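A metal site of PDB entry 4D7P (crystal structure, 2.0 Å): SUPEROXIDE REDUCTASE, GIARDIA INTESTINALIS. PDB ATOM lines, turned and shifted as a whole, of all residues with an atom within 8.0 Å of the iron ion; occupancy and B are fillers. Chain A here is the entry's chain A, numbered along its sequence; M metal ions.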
ATOM      1  N   GLU A  17      14.682   3.862  24.906  1.00  0.00           N
ATOM      2  CA  GLU A  17      15.875   4.425  25.567  1.00  0.00           C
ATOM      3  C   GLU A  17      15.575   5.852  26.045  1.00  0.00           C
ATOM      4  O   GLU A  17      14.909   6.625  25.345  1.00  0.00           O
ATOM      5  CB  GLU A  17      17.071   4.409  24.594  1.00  0.00           C
ATOM      6  CG  GLU A  17      18.374   4.990  25.142  1.00  0.00           C
ATOM      7  CD  GLU A  17      19.485   5.029  24.098  1.00  0.00           C
ATOM      8  OE1 GLU A  17      19.900   3.940  23.633  1.00  0.00           O
ATOM      9  OE2 GLU A  17      19.951   6.138  23.751  1.00  0.00           O
ATOM     10  N   LYS A  18      16.054   6.192  27.252  1.00  0.00           N
ATOM     11  CA  LYS A  18      15.666   7.466  27.864  1.00  0.00           C
ATOM     12  C   LYS A  18      16.863   8.396  28.098  1.00  0.00           C
ATOM     13  O   LYS A  18      17.897   7.992  28.623  1.00  0.00           O
ATOM     14  CB  LYS A  18      14.930   7.221  29.182  1.00  0.00           C
ATOM     15  CG  LYS A  18      13.796   6.188  29.101  1.00  0.00           C
ATOM     16  CD  LYS A  18      12.654   6.634  28.193  1.00  0.00           C
ATOM     17  CE  LYS A  18      11.519   5.596  28.182  1.00  0.00           C
ATOM     18  NZ  LYS A  18      10.341   5.992  27.358  1.00  0.00           N
ATOM     19  N   HIS A  19      16.693   9.644  27.693  1.00  0.00           N
ATOM     20  CA  HIS A  19      17.727  10.653  27.818  1.00  0.00           C
ATOM     21  C   HIS A  19      17.300  11.756  28.806  1.00  0.00           C
ATOM     22  O   HIS A  19      18.123  12.502  29.317  1.00  0.00           O
ATOM     23  CB  HIS A  19      18.048  11.287  26.445  1.00  0.00           C
ATOM     24  CG  HIS A  19      18.795  10.408  25.487  1.00  0.00           C
ATOM     25  ND1 HIS A  19      18.163   9.539  24.618  1.00  0.00           N
ATOM     26  CD2 HIS A  19      20.117  10.329  25.184  1.00  0.00           C
ATOM     27  CE1 HIS A  19      19.057   8.930  23.865  1.00  0.00           C
ATOM     28  NE2 HIS A  19      20.258   9.403  24.175  1.00  0.00           N
ATOM     29  N   HIS A  40      20.336   5.568  31.018  1.00  0.00           N
ATOM     30  CA  HIS A  40      20.943   5.663  29.695  1.00  0.00           C
ATOM     31  C   HIS A  40      22.277   4.926  29.641  1.00  0.00           C
ATOM     32  O   HIS A  40      22.961   4.855  30.655  1.00  0.00           O
ATOM     33  CB  HIS A  40      21.136   7.133  29.312  1.00  0.00           C
ATOM     34  CG  HIS A  40      21.737   7.349  27.958  1.00  0.00           C
ATOM     35  ND1 HIS A  40      23.096   7.250  27.719  1.00  0.00           N
ATOM     36  CD2 HIS A  40      21.170   7.697  26.783  1.00  0.00           C
ATOM     37  CE1 HIS A  40      23.329   7.519  26.446  1.00  0.00           C
ATOM     38  NE2 HIS A  40      22.180   7.798  25.855  1.00  0.00           N
ATOM     39  N   PRO A  41      22.633   4.347  28.486  1.00  0.00           N
ATOM     40  CA  PRO A  41      23.940   3.703  28.364  1.00  0.00           C
ATOM     41  C   PRO A  41      25.134   4.583  28.727  1.00  0.00           C
ATOM     42  O   PRO A  41      25.101   5.819  28.675  1.00  0.00           O
ATOM     43  CB  PRO A  41      23.992   3.311  26.881  1.00  0.00           C
ATOM     44  CG  PRO A  41      22.568   3.021  26.551  1.00  0.00           C
ATOM     45  CD  PRO A  41      21.763   4.050  27.332  1.00  0.00           C
ATOM     46  N   LYS A  45      31.578   4.672  23.310  1.00  0.00           N
ATOM     47  CA  LYS A  45      31.039   5.109  22.023  1.00  0.00           C
ATOM     48  C   LYS A  45      29.604   5.649  22.141  1.00  0.00           C
ATOM     49  O   LYS A  45      29.095   6.260  21.206  1.00  0.00           O
ATOM     50  CB  LYS A  45      31.097   3.960  21.004  1.00  0.00           C
ATOM     51  CG  LYS A  45      32.513   3.550  20.610  1.00  0.00           C
ATOM     52  CD  LYS A  45      32.494   2.368  19.634  1.00  0.00           C
ATOM     53  CE  LYS A  45      33.897   1.840  19.406  1.00  0.00           C
ATOM     54  NZ  LYS A  45      34.816   2.897  18.892  1.00  0.00           N
ATOM     55  N   HIS A  46      28.967   5.418  23.289  1.00  0.00           N
ATOM     56  CA  HIS A  46      27.631   5.983  23.526  1.00  0.00           C
ATOM     57  C   HIS A  46      27.499   6.417  24.981  1.00  0.00           C
ATOM     58  O   HIS A  46      27.553   5.583  25.900  1.00  0.00           O
ATOM     59  CB  HIS A  46      26.530   4.968  23.173  1.00  0.00           C
ATOM     60  CG  HIS A  46      25.138   5.542  23.262  1.00  0.00           C
ATOM     61  ND1 HIS A  46      24.021   4.746  23.397  1.00  0.00           N
ATOM     62  CD2 HIS A  46      24.698   6.822  23.218  1.00  0.00           C
ATOM     63  CE1 HIS A  46      22.939   5.512  23.427  1.00  0.00           C
ATOM     64  NE2 HIS A  46      23.322   6.772  23.330  1.00  0.00           N
ATOM     65  N   TYR A  47      27.327   7.712  25.187  1.00  0.00           N
ATOM     66  CA  TYR A  47      27.385   8.258  26.541  1.00  0.00           C
ATOM     67  C   TYR A  47      26.625   9.564  26.677  1.00  0.00           C
ATOM     68  O   TYR A  47      26.467  10.302  25.706  1.00  0.00           O
ATOM     69  CB  TYR A  47      28.842   8.462  26.948  1.00  0.00           C
ATOM     70  CG  TYR A  47      29.657   9.313  25.981  1.00  0.00           C
ATOM     71  CD1 TYR A  47      29.727  10.692  26.145  1.00  0.00           C
ATOM     72  CD2 TYR A  47      30.371   8.748  24.931  1.00  0.00           C
ATOM     73  CE1 TYR A  47      30.465  11.488  25.282  1.00  0.00           C
ATOM     74  CE2 TYR A  47      31.128   9.548  24.043  1.00  0.00           C
ATOM     75  CZ  TYR A  47      31.167  10.914  24.246  1.00  0.00           C
ATOM     76  OH  TYR A  47      31.902  11.746  23.419  1.00  0.00           O
ATOM     77  N   ILE A  48      26.125   9.830  27.870  1.00  0.00           N
ATOM     78  CA  ILE A  48      25.732  11.183  28.217  1.00  0.00           C
ATOM     79  C   ILE A  48      26.949  11.784  28.895  1.00  0.00           C
ATOM     80  O   ILE A  48      27.403  11.319  29.951  1.00  0.00           O
ATOM     81  CB  ILE A  48      24.486  11.243  29.100  1.00  0.00           C
ATOM     82  CG1 ILE A  48      23.243  11.009  28.235  1.00  0.00           C
ATOM     83  CG2 ILE A  48      24.380  12.597  29.807  1.00  0.00           C
ATOM     84  CD1 ILE A  48      21.984  10.745  29.058  1.00  0.00           C
ATOM     85  N   TYR A  98      23.394  15.886  27.669  1.00  0.00           N
ATOM     86  CA  TYR A  98      23.958  15.781  26.326  1.00  0.00           C
ATOM     87  C   TYR A  98      24.445  14.363  26.051  1.00  0.00           C
ATOM     88  O   TYR A  98      25.341  13.867  26.734  1.00  0.00           O
ATOM     89  CB  TYR A  98      25.128  16.769  26.125  1.00  0.00           C
ATOM     90  CG  TYR A  98      26.066  16.345  25.010  1.00  0.00           C
ATOM     91  CD1 TYR A  98      25.658  16.410  23.671  1.00  0.00           C
ATOM     92  CD2 TYR A  98      27.349  15.871  25.278  1.00  0.00           C
ATOM     93  CE1 TYR A  98      26.499  16.012  22.636  1.00  0.00           C
ATOM     94  CE2 TYR A  98      28.204  15.474  24.241  1.00  0.00           C
ATOM     95  CZ  TYR A  98      27.768  15.546  22.926  1.00  0.00           C
ATOM     96  OH  TYR A  98      28.587  15.148  21.886  1.00  0.00           O
ATOM     97  N   CYS A  99      23.855  13.720  25.054  1.00  0.00           N
ATOM     98  CA  CYS A  99      24.314  12.405  24.612  1.00  0.00           C
ATOM     99  C   CYS A  99      25.033  12.563  23.281  1.00  0.00           C
ATOM    100  O   CYS A  99      24.548  13.269  22.385  1.00  0.00           O
ATOM    101  CB  CYS A  99      23.142  11.447  24.472  1.00  0.00           C
ATOM    102  SG  CYS A  99      23.524   9.955  23.530  1.00  0.00           S
ATOM    103  N   ASN A 100      26.176  11.902  23.136  1.00  0.00           N
ATOM    104  CA  ASN A 100      26.976  12.107  21.923  1.00  0.00           C
ATOM    105  C   ASN A 100      26.203  11.655  20.694  1.00  0.00           C
ATOM    106  O   ASN A 100      26.261  12.299  19.645  1.00  0.00           O
ATOM    107  CB  ASN A 100      28.313  11.372  22.008  1.00  0.00           C
ATOM    108  CG  ASN A 100      28.152   9.866  21.992  1.00  0.00           C
ATOM    109  OD1 ASN A 100      27.349   9.301  22.739  1.00  0.00           O
ATOM    110  ND2 ASN A 100      28.917   9.199  21.131  1.00  0.00           N
ATOM    111  N   LEU A 101      25.444  10.566  20.806  1.00  0.00           N
ATOM    112  CA  LEU A 101      24.749  10.054  19.638  1.00  0.00           C
ATOM    113  C   LEU A 101      23.431  10.786  19.418  1.00  0.00           C
ATOM    114  O   LEU A 101      23.020  10.971  18.275  1.00  0.00           O
ATOM    115  CB  LEU A 101      24.499   8.548  19.767  1.00  0.00           C
ATOM    116  CG  LEU A 101      25.749   7.663  19.734  1.00  0.00           C
ATOM    117  CD1 LEU A 101      25.371   6.191  19.861  1.00  0.00           C
ATOM    118  CD2 LEU A 101      26.553   7.903  18.459  1.00  0.00           C
ATOM    119  N   HIS A 102      22.789  11.220  20.490  1.00  0.00           N
ATOM    120  CA  HIS A 102      21.384  11.634  20.388  1.00  0.00           C
ATOM    121  C   HIS A 102      21.083  13.065  20.779  1.00  0.00           C
ATOM    122  O   HIS A 102      19.919  13.457  20.862  1.00  0.00           O
ATOM    123  CB  HIS A 102      20.531  10.677  21.207  1.00  0.00           C
ATOM    124  CG  HIS A 102      20.622   9.264  20.746  1.00  0.00           C
ATOM    125  ND1 HIS A 102      20.840   8.211  21.592  1.00  0.00           N
ATOM    126  CD2 HIS A 102      20.562   8.732  19.489  1.00  0.00           C
ATOM    127  CE1 HIS A 102      20.905   7.089  20.895  1.00  0.00           C
ATOM    128  NE2 HIS A 102      20.733   7.376  19.616  1.00  0.00           N
ATOM    129  N   GLY A 103      22.128  13.860  20.997  1.00  0.00           N
ATOM    130  CA  GLY A 103      21.946  15.277  21.230  1.00  0.00           C
ATOM    131  C   GLY A 103      21.467  15.645  22.615  1.00  0.00           C
ATOM    132  O   GLY A 103      21.582  14.843  23.549  1.00  0.00           O
ATOM    133  N   TRP A 105      18.872  16.843  25.702  1.00  0.00           N
ATOM    134  CA  TRP A 105      17.514  16.586  26.186  1.00  0.00           C
ATOM    135  C   TRP A 105      17.287  17.369  27.455  1.00  0.00           C
ATOM    136  O   TRP A 105      18.063  17.275  28.403  1.00  0.00           O
ATOM    137  CB  TRP A 105      17.306  15.094  26.422  1.00  0.00           C
ATOM    138  CG  TRP A 105      17.406  14.310  25.172  1.00  0.00           C
ATOM    139  CD1 TRP A 105      18.546  13.969  24.502  1.00  0.00           C
ATOM    140  CD2 TRP A 105      16.322  13.748  24.429  1.00  0.00           C
ATOM    141  NE1 TRP A 105      18.233  13.232  23.377  1.00  0.00           N
ATOM    142  CE2 TRP A 105      16.866  13.086  23.313  1.00  0.00           C
ATOM    143  CE3 TRP A 105      14.930  13.744  24.600  1.00  0.00           C
ATOM    144  CZ2 TRP A 105      16.088  12.431  22.363  1.00  0.00           C
ATOM    145  CZ3 TRP A 105      14.151  13.097  23.656  1.00  0.00           C
ATOM    146  CH2 TRP A 105      14.724  12.442  22.555  1.00  0.00           C
HETATM  147 FE    FE M   1      21.872   8.255  23.696  1.00  0.00          FE
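A ring nitrogen (NE2) of His 19 sits close to the side-chain carboxylate (OE2) of Glu 17. The side-chain carboxylate (OE2) of Glu 17 sits close to a ring nitrogen (NE2) of His 46. A ring nitrogen (NE2) of His 40 lies close to the side-chain carboxylate (OE2) of Glu 17, 3.5 Å away. OE2 of Glu 17 lies close to ND1 of His 102 (3.1 Å). The indole nitrogen (NE1) of Trp 105 lies within hydrogen-bond range of the backbone carbonyl oxygen (O) of His 102. N of Leu 101 sits close to SG of Cys 99. The side-chain sulfur of Cys 99 sits close to the backbone carbonyl oxygen of Tyr 47 (3.7 Å).
Glu 17 touches the iron ion. Six residues have an atom within 4 Å of the iron ion: Glu 17, His 19, His 40, His 46, Cys 99 and His 102. The nearest printed residue that does not touch the iron ion is Leu 101 (4.7 Å).
The iron ion is bound by a ring nitrogen (NE2) of His 19 (2.0 Å), a ring nitrogen (NE2) of His 46 (2.1 Å), a ring nitrogen (NE2) of His 40 (2.2 Å), a ring nitrogen (ND1) of His 102 (2.3 Å) and the side-chain sulfur (SG) of Cys 99 (2.4 Å). The iron ion has five donor atoms within binding distance.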
